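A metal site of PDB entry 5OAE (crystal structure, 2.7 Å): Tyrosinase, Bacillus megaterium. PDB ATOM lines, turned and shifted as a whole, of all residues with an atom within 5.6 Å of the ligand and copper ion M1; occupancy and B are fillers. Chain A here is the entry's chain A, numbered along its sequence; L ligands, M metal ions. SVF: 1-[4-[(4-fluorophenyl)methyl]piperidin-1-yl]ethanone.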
ATOM      1  N   HIS A  39     -26.879 -11.177  23.310  1.00  0.00           N
ATOM      2  CA  HIS A  39     -25.576 -10.684  23.722  1.00  0.00           C
ATOM      3  C   HIS A  39     -24.450 -11.461  23.060  1.00  0.00           C
ATOM      4  O   HIS A  39     -23.490 -10.875  22.554  1.00  0.00           O
ATOM      5  CB  HIS A  39     -25.441 -10.757  25.247  1.00  0.00           C
ATOM      6  CG  HIS A  39     -24.180 -10.152  25.771  1.00  0.00           C
ATOM      7  ND1 HIS A  39     -23.101 -10.905  26.174  1.00  0.00           N
ATOM      8  CD2 HIS A  39     -23.839  -8.862  25.997  1.00  0.00           C
ATOM      9  CE1 HIS A  39     -22.140 -10.105  26.602  1.00  0.00           C
ATOM     10  NE2 HIS A  39     -22.563  -8.862  26.503  1.00  0.00           N
ATOM     11  N   ALA A  56     -21.450  -5.352  19.735  1.00  0.00           N
ATOM     12  CA  ALA A  56     -21.744  -4.982  21.110  1.00  0.00           C
ATOM     13  C   ALA A  56     -20.517  -4.579  21.911  1.00  0.00           C
ATOM     14  O   ALA A  56     -20.643  -3.946  22.965  1.00  0.00           O
ATOM     15  CB  ALA A  56     -22.457  -6.131  21.805  1.00  0.00           C
ATOM     16  N   HIS A  57     -19.329  -4.944  21.438  1.00  0.00           N
ATOM     17  CA  HIS A  57     -18.120  -4.706  22.224  1.00  0.00           C
ATOM     18  C   HIS A  57     -16.920  -4.253  21.398  1.00  0.00           C
ATOM     19  O   HIS A  57     -16.928  -4.327  20.168  1.00  0.00           O
ATOM     20  CB  HIS A  57     -17.732  -5.965  22.995  1.00  0.00           C
ATOM     21  CG  HIS A  57     -18.863  -6.560  23.794  1.00  0.00           C
ATOM     22  ND1 HIS A  57     -19.673  -7.555  23.301  1.00  0.00           N
ATOM     23  CD2 HIS A  57     -19.309  -6.280  25.039  1.00  0.00           C
ATOM     24  CE1 HIS A  57     -20.570  -7.875  24.216  1.00  0.00           C
ATOM     25  NE2 HIS A  57     -20.379  -7.120  25.280  1.00  0.00           N
ATOM     26  N   PHE A  62     -20.417   0.162  21.874  1.00  0.00           N
ATOM     27  CA  PHE A  62     -20.458  -0.596  23.125  1.00  0.00           C
ATOM     28  C   PHE A  62     -21.464  -0.022  24.119  1.00  0.00           C
ATOM     29  O   PHE A  62     -22.226  -0.763  24.734  1.00  0.00           O
ATOM     30  CB  PHE A  62     -19.071  -0.625  23.768  1.00  0.00           C
ATOM     31  CG  PHE A  62     -19.087  -0.964  25.227  1.00  0.00           C
ATOM     32  CD1 PHE A  62     -19.354  -2.254  25.656  1.00  0.00           C
ATOM     33  CD2 PHE A  62     -18.823   0.009  26.187  1.00  0.00           C
ATOM     34  CE1 PHE A  62     -19.371  -2.562  27.012  1.00  0.00           C
ATOM     35  CE2 PHE A  62     -18.836  -0.292  27.528  1.00  0.00           C
ATOM     36  CZ  PHE A  62     -19.109  -1.576  27.945  1.00  0.00           C
ATOM     37  N   TRP A  65     -25.396   0.126  22.680  1.00  0.00           N
ATOM     38  CA  TRP A  65     -25.911  -1.234  22.536  1.00  0.00           C
ATOM     39  C   TRP A  65     -26.469  -1.716  23.870  1.00  0.00           C
ATOM     40  O   TRP A  65     -27.603  -2.167  23.954  1.00  0.00           O
ATOM     41  CB  TRP A  65     -24.819  -2.183  22.049  1.00  0.00           C
ATOM     42  CG  TRP A  65     -25.324  -3.521  21.599  1.00  0.00           C
ATOM     43  CD1 TRP A  65     -25.592  -3.903  20.308  1.00  0.00           C
ATOM     44  CD2 TRP A  65     -25.610  -4.662  22.421  1.00  0.00           C
ATOM     45  NE1 TRP A  65     -26.036  -5.210  20.290  1.00  0.00           N
ATOM     46  CE2 TRP A  65     -26.054  -5.690  21.562  1.00  0.00           C
ATOM     47  CE3 TRP A  65     -25.546  -4.907  23.793  1.00  0.00           C
ATOM     48  CZ2 TRP A  65     -26.424  -6.946  22.052  1.00  0.00           C
ATOM     49  CZ3 TRP A  65     -25.911  -6.156  24.268  1.00  0.00           C
ATOM     50  CH2 TRP A  65     -26.345  -7.153  23.392  1.00  0.00           C
ATOM     51  N   HIS A  66     -25.650  -1.610  24.910  1.00  0.00           N
ATOM     52  CA  HIS A  66     -26.029  -2.098  26.226  1.00  0.00           C
ATOM     53  C   HIS A  66     -27.116  -1.230  26.860  1.00  0.00           C
ATOM     54  O   HIS A  66     -27.873  -1.708  27.699  1.00  0.00           O
ATOM     55  CB  HIS A  66     -24.805  -2.177  27.132  1.00  0.00           C
ATOM     56  CG  HIS A  66     -23.855  -3.267  26.747  1.00  0.00           C
ATOM     57  ND1 HIS A  66     -22.853  -3.086  25.814  1.00  0.00           N
ATOM     58  CD2 HIS A  66     -23.760  -4.561  27.159  1.00  0.00           C
ATOM     59  CE1 HIS A  66     -22.171  -4.219  25.676  1.00  0.00           C
ATOM     60  NE2 HIS A  66     -22.701  -5.122  26.481  1.00  0.00           N
ATOM     61  N   GLY A 193     -12.787  -0.464  29.219  1.00  0.00           N
ATOM     62  CA  GLY A 193     -11.709  -0.950  30.061  1.00  0.00           C
ATOM     63  C   GLY A 193     -10.522  -1.543  29.336  1.00  0.00           C
ATOM     64  O   GLY A 193      -9.869  -2.454  29.856  1.00  0.00           O
ATOM     65  N   PHE A 194     -10.229  -1.054  28.136  1.00  0.00           N
ATOM     66  CA  PHE A 194      -9.100  -1.577  27.376  1.00  0.00           C
ATOM     67  C   PHE A 194      -7.852  -0.717  27.557  1.00  0.00           C
ATOM     68  O   PHE A 194      -6.763  -1.097  27.131  1.00  0.00           O
ATOM     69  CB  PHE A 194      -9.475  -1.705  25.895  1.00  0.00           C
ATOM     70  CG  PHE A 194     -10.455  -2.800  25.621  1.00  0.00           C
ATOM     71  CD1 PHE A 194     -10.102  -4.132  25.779  1.00  0.00           C
ATOM     72  CD2 PHE A 194     -11.743  -2.503  25.194  1.00  0.00           C
ATOM     73  CE1 PHE A 194     -11.003  -5.142  25.524  1.00  0.00           C
ATOM     74  CE2 PHE A 194     -12.654  -3.515  24.942  1.00  0.00           C
ATOM     75  CZ  PHE A 194     -12.280  -4.840  25.102  1.00  0.00           C
ATOM     76  N   GLY A 197      -5.964  -2.477  30.279  1.00  0.00           N
ATOM     77  CA  GLY A 197      -6.979  -3.365  30.785  1.00  0.00           C
ATOM     78  C   GLY A 197      -6.427  -4.572  31.529  1.00  0.00           C
ATOM     79  O   GLY A 197      -5.234  -4.859  31.450  1.00  0.00           O
ATOM     80  N   PRO A 198      -7.301  -5.272  32.239  1.00  0.00           N
ATOM     81  CA  PRO A 198      -8.716  -4.900  32.315  1.00  0.00           C
ATOM     82  C   PRO A 198      -8.961  -3.814  33.357  1.00  0.00           C
ATOM     83  O   PRO A 198      -8.356  -3.840  34.428  1.00  0.00           O
ATOM     84  CB  PRO A 198      -9.397  -6.198  32.736  1.00  0.00           C
ATOM     85  CG  PRO A 198      -8.354  -6.939  33.506  1.00  0.00           C
ATOM     86  CD  PRO A 198      -7.042  -6.595  32.839  1.00  0.00           C
ATOM     87  N   GLN A 199      -9.844  -2.885  33.069  1.00  0.00           N
ATOM     88  CA  GLN A 199     -10.165  -1.848  34.031  1.00  0.00           C
ATOM     89  C   GLN A 199     -11.630  -1.481  33.944  1.00  0.00           C
ATOM     90  O   GLN A 199     -12.263  -1.718  32.961  1.00  0.00           O
ATOM     91  CB  GLN A 199      -9.267  -0.643  33.855  1.00  0.00           C
ATOM     92  CG  GLN A 199      -7.800  -0.999  33.779  1.00  0.00           C
ATOM     93  CD  GLN A 199      -7.089  -0.856  35.095  1.00  0.00           C
ATOM     94  OE1 GLN A 199      -7.661  -0.399  36.065  1.00  0.00           O
ATOM     95  NE2 GLN A 199      -5.840  -1.261  35.139  1.00  0.00           N
ATOM     96  N   HIS A 201     -15.323  -1.404  33.648  1.00  0.00           N
ATOM     97  CA  HIS A 201     -16.268  -2.402  33.140  1.00  0.00           C
ATOM     98  C   HIS A 201     -15.626  -3.769  32.899  1.00  0.00           C
ATOM     99  O   HIS A 201     -16.148  -4.786  33.356  1.00  0.00           O
ATOM    100  CB  HIS A 201     -16.913  -1.889  31.852  1.00  0.00           C
ATOM    101  CG  HIS A 201     -17.552  -2.966  31.026  1.00  0.00           C
ATOM    102  ND1 HIS A 201     -16.937  -3.519  29.926  1.00  0.00           N
ATOM    103  CD2 HIS A 201     -18.749  -3.573  31.128  1.00  0.00           C
ATOM    104  CE1 HIS A 201     -17.726  -4.425  29.389  1.00  0.00           C
ATOM    105  NE2 HIS A 201     -18.834  -4.483  30.098  1.00  0.00           N
ATOM    106  N   ASN A 202     -14.503  -3.795  32.188  1.00  0.00           N
ATOM    107  CA  ASN A 202     -13.823  -5.043  31.873  1.00  0.00           C
ATOM    108  C   ASN A 202     -13.262  -5.729  33.115  1.00  0.00           C
ATOM    109  O   ASN A 202     -13.246  -6.957  33.206  1.00  0.00           O
ATOM    110  CB  ASN A 202     -12.699  -4.808  30.858  1.00  0.00           C
ATOM    111  CG  ASN A 202     -13.221  -4.534  29.465  1.00  0.00           C
ATOM    112  OD1 ASN A 202     -14.397  -4.775  29.166  1.00  0.00           O
ATOM    113  ND2 ASN A 202     -12.353  -4.036  28.584  1.00  0.00           N
ATOM    114  N   ARG A 203     -12.797  -4.928  34.065  1.00  0.00           N
ATOM    115  CA  ARG A 203     -12.235  -5.449  35.304  1.00  0.00           C
ATOM    116  C   ARG A 203     -13.294  -6.095  36.181  1.00  0.00           C
ATOM    117  O   ARG A 203     -13.055  -7.116  36.816  1.00  0.00           O
ATOM    118  CB  ARG A 203     -11.524  -4.334  36.080  1.00  0.00           C
ATOM    119  CG  ARG A 203     -10.980  -4.746  37.435  1.00  0.00           C
ATOM    120  CD  ARG A 203     -10.209  -3.621  38.087  1.00  0.00           C
ATOM    121  NE  ARG A 203      -8.886  -3.427  37.492  1.00  0.00           N
ATOM    122  CZ  ARG A 203      -7.761  -3.871  38.020  1.00  0.00           C
ATOM    123  NH1 ARG A 203      -7.782  -4.523  39.174  1.00  0.00           N
ATOM    124  NH2 ARG A 203      -6.600  -3.655  37.408  1.00  0.00           N
ATOM    125  N   HIS A 205     -16.022  -7.591  35.194  1.00  0.00           N
ATOM    126  CA  HIS A 205     -16.327  -8.894  34.602  1.00  0.00           C
ATOM    127  C   HIS A 205     -15.320  -9.930  35.080  1.00  0.00           C
ATOM    128  O   HIS A 205     -15.695 -10.993  35.591  1.00  0.00           O
ATOM    129  CB  HIS A 205     -16.311  -8.818  33.075  1.00  0.00           C
ATOM    130  CG  HIS A 205     -17.593  -8.326  32.472  1.00  0.00           C
ATOM    131  ND1 HIS A 205     -18.737  -9.095  32.435  1.00  0.00           N
ATOM    132  CD2 HIS A 205     -17.917  -7.150  31.887  1.00  0.00           C
ATOM    133  CE1 HIS A 205     -19.707  -8.410  31.859  1.00  0.00           C
ATOM    134  NE2 HIS A 205     -19.236  -7.227  31.516  1.00  0.00           N
ATOM    135  N   ARG A 206     -14.038  -9.635  34.883  1.00  0.00           N
ATOM    136  CA  ARG A 206     -12.969 -10.552  35.268  1.00  0.00           C
ATOM    137  C   ARG A 206     -12.910 -10.800  36.768  1.00  0.00           C
ATOM    138  O   ARG A 206     -12.509 -11.870  37.206  1.00  0.00           O
ATOM    139  CB  ARG A 206     -11.617 -10.019  34.768  1.00  0.00           C
ATOM    140  CG  ARG A 206     -11.531  -9.873  33.258  1.00  0.00           C
ATOM    141  CD  ARG A 206     -10.499 -10.831  32.668  1.00  0.00           C
ATOM    142  NE  ARG A 206      -9.658 -10.181  31.674  1.00  0.00           N
ATOM    143  CZ  ARG A 206      -8.475 -10.640  31.287  1.00  0.00           C
ATOM    144  NH1 ARG A 206      -7.990 -11.755  31.810  1.00  0.00           N
ATOM    145  NH2 ARG A 206      -7.770  -9.973  30.372  1.00  0.00           N
ATOM    146  N   MET A 212     -19.339 -14.662  34.105  1.00  0.00           N
ATOM    147  CA  MET A 212     -19.089 -13.242  33.919  1.00  0.00           C
ATOM    148  C   MET A 212     -17.681 -12.979  33.382  1.00  0.00           C
ATOM    149  O   MET A 212     -17.362 -11.863  32.978  1.00  0.00           O
ATOM    150  CB  MET A 212     -19.280 -12.486  35.234  1.00  0.00           C
ATOM    151  CG  MET A 212     -20.723 -12.341  35.675  1.00  0.00           C
ATOM    152  SD  MET A 212     -21.593 -10.984  34.849  1.00  0.00           S
ATOM    153  CE  MET A 212     -20.599  -9.585  35.362  1.00  0.00           C
ATOM    154  N   GLY A 213     -16.852 -14.017  33.361  1.00  0.00           N
ATOM    155  CA  GLY A 213     -15.470 -13.858  32.933  1.00  0.00           C
ATOM    156  C   GLY A 213     -15.329 -13.837  31.426  1.00  0.00           C
ATOM    157  O   GLY A 213     -14.341 -13.313  30.904  1.00  0.00           O
ATOM    158  N   VAL A 214     -16.312 -14.387  30.716  1.00  0.00           N
ATOM    159  CA  VAL A 214     -16.282 -14.401  29.268  1.00  0.00           C
ATOM    160  C   VAL A 214     -17.529 -13.745  28.664  1.00  0.00           C
ATOM    161  O   VAL A 214     -18.579 -13.690  29.296  1.00  0.00           O
ATOM    162  CB  VAL A 214     -16.144 -15.850  28.718  1.00  0.00           C
ATOM    163  CG1 VAL A 214     -14.953 -16.546  29.356  1.00  0.00           C
ATOM    164  CG2 VAL A 214     -17.415 -16.627  28.971  1.00  0.00           C
ATOM    165  N   VAL A 215     -17.389 -13.232  27.443  1.00  0.00           N
ATOM    166  CA  VAL A 215     -18.461 -12.480  26.802  1.00  0.00           C
ATOM    167  C   VAL A 215     -19.754 -13.272  26.504  1.00  0.00           C
ATOM    168  O   VAL A 215     -20.829 -12.842  26.903  1.00  0.00           O
ATOM    169  CB  VAL A 215     -17.959 -11.847  25.477  1.00  0.00           C
ATOM    170  CG1 VAL A 215     -19.086 -11.099  24.775  1.00  0.00           C
ATOM    171  CG2 VAL A 215     -16.784 -10.922  25.754  1.00  0.00           C
ATOM    172  N   ALA A 218     -21.756 -14.322  29.825  1.00  0.00           N
ATOM    173  CA  ALA A 218     -21.868 -13.329  30.890  1.00  0.00           C
ATOM    174  C   ALA A 218     -23.311 -13.068  31.383  1.00  0.00           C
ATOM    175  O   ALA A 218     -23.535 -12.963  32.590  1.00  0.00           O
ATOM    176  CB  ALA A 218     -21.226 -12.026  30.455  1.00  0.00           C
ATOM    177  N   PHE A 224     -25.066  -9.261  35.859  1.00  0.00           N
ATOM    178  CA  PHE A 224     -24.654  -8.657  34.597  1.00  0.00           C
ATOM    179  C   PHE A 224     -25.470  -7.405  34.296  1.00  0.00           C
ATOM    180  O   PHE A 224     -24.971  -6.444  33.724  1.00  0.00           O
ATOM    181  CB  PHE A 224     -24.796  -9.678  33.451  1.00  0.00           C
ATOM    182  CG  PHE A 224     -24.430  -9.141  32.095  1.00  0.00           C
ATOM    183  CD1 PHE A 224     -23.125  -9.212  31.642  1.00  0.00           C
ATOM    184  CD2 PHE A 224     -25.396  -8.583  31.268  1.00  0.00           C
ATOM    185  CE1 PHE A 224     -22.785  -8.724  30.394  1.00  0.00           C
ATOM    186  CE2 PHE A 224     -25.056  -8.096  30.020  1.00  0.00           C
ATOM    187  CZ  PHE A 224     -23.758  -8.164  29.579  1.00  0.00           C
ATOM    188  N   HIS A 228     -24.060  -3.436  34.262  1.00  0.00           N
ATOM    189  CA  HIS A 228     -24.169  -2.551  33.104  1.00  0.00           C
ATOM    190  C   HIS A 228     -25.077  -1.358  33.364  1.00  0.00           C
ATOM    191  O   HIS A 228     -24.988  -0.342  32.678  1.00  0.00           O
ATOM    192  CB  HIS A 228     -24.653  -3.339  31.883  1.00  0.00           C
ATOM    193  CG  HIS A 228     -23.561  -4.075  31.180  1.00  0.00           C
ATOM    194  ND1 HIS A 228     -22.811  -3.503  30.167  1.00  0.00           N
ATOM    195  CD2 HIS A 228     -23.069  -5.317  31.348  1.00  0.00           C
ATOM    196  CE1 HIS A 228     -21.915  -4.369  29.748  1.00  0.00           C
ATOM    197  NE2 HIS A 228     -22.056  -5.484  30.448  1.00  0.00           N
HETATM  198  C01 SVF L   1     -18.221  -9.870  29.191  1.00  0.00           C
HETATM  199  C02 SVF L   1     -19.388  -9.295  28.699  1.00  0.00           C
HETATM  200  C03 SVF L   1     -17.030  -9.167  29.118  1.00  0.00           C
HETATM  201  C04 SVF L   1     -19.331  -8.042  28.157  1.00  0.00           C
HETATM  202  C05 SVF L   1     -16.992  -7.905  28.556  1.00  0.00           C
HETATM  203  C06 SVF L   1     -18.157  -7.339  28.067  1.00  0.00           C
HETATM  204  C08 SVF L   1     -15.758  -9.759  29.564  1.00  0.00           C
HETATM  205  C09 SVF L   1     -14.564  -9.219  28.905  1.00  0.00           C
HETATM  206  C10 SVF L   1     -13.504 -10.293  28.762  1.00  0.00           C
HETATM  207  C11 SVF L   1     -13.985  -8.048  29.674  1.00  0.00           C
HETATM  208  C12 SVF L   1     -12.298  -9.729  28.033  1.00  0.00           C
HETATM  209  C13 SVF L   1     -12.789  -7.498  28.943  1.00  0.00           C
HETATM  210  N14 SVF L   1     -11.796  -8.572  28.764  1.00  0.00           N
HETATM  211  C15 SVF L   1     -10.464  -8.336  28.871  1.00  0.00           C
HETATM  212  O16 SVF L   1      -9.660  -8.961  28.207  1.00  0.00           O
HETATM  213  C17 SVF L   1     -10.003  -7.069  29.544  1.00  0.00           C
HETATM  214  F07 SVF L   1     -20.474  -7.481  27.664  1.00  0.00           F
HETATM  215 CU    CU M   1     -22.014  -6.963  26.621  1.00  0.00          CU
HETATM  216 CU    CU M   2     -20.162  -6.066  30.193  1.00  0.00          CU
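The guanidinium group of Arg 206 is in hydrogen-bond range of an oxygen (O16) of the ligand, at 3.0 Å.
ND1 of His 66 is in hydrogen-bond range of O of Phe 62, 2.6 Å away.
ND1 of His 39 sits close to O of Val 215, at 3.1 Å.
ND1 of His 201 lies within hydrogen-bond range of OD1 of Asn 202, at 2.9 Å.
The backbone carbonyl oxygen of Gly 193 sits close to the side-chain amide nitrogen of Asn 202 (3.2 Å).
A ring nitrogen (ND1) of His 205 sits at hydrogen-bond distance from the backbone carbonyl oxygen (O) of Met 212 (3.1 Å).
O of Pro 198 is in hydrogen-bond range of NE of Arg 203 (3.1 Å).
Pro 198 touches the ligand.
His 201 touches the ligand (CE1 to C06, 3.2 Å).
Asn 202 touches the ligand.
CE1 of His 205 touches C02 of the ligand (3.3 Å).
Gly 213 touches the ligand.
Val 214 touches the ligand.
Val 215 touches the ligand (CA to C01, 3.5 Å).
CB of Ala 218 touches C02 of the ligand, 3.7 Å away.
Phe 224 touches the ligand.
His 228 touches the ligand (NE2 to F07, 3.8 Å).
Hydrophobic or aromatic side chains within 4 Å of the ligand: His 39, His 57, Pro 198, His 201, His 205, Val 215, Ala 218 and Phe 224.
Within 4 Å of the ligand: His 39, His 57, His 66, Pro 198, His 201, Asn 202, His 205, Arg 206, Gly 213, Val 214, Val 215, Ala 218, Phe 224 and His 228.
The nearest printed residue that does not touch the ligand is Met 212 (4.3 Å).
Residues that only touch copper ion M1: Phe 224.
Four residues have an atom within 4 Å of copper ion M1: His 39, His 57, His 66 and Phe 224.
Along chain A the residues within 4 Å of copper ion M1 span positions 39 to 224.
The nearest printed residue that does not touch copper ion M1 is His 228 (4.1 Å).
Copper ion M1 is bound by a fluorine (F07) of the ligand (1.9 Å), a ring nitrogen (NE2) of His 66 (2.0 Å), a ring nitrogen (NE2) of His 39 (2.0 Å) and a ring nitrogen (NE2) of His 57 (2.1 Å).
Copper ion M1 has four donor atoms within binding distance.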
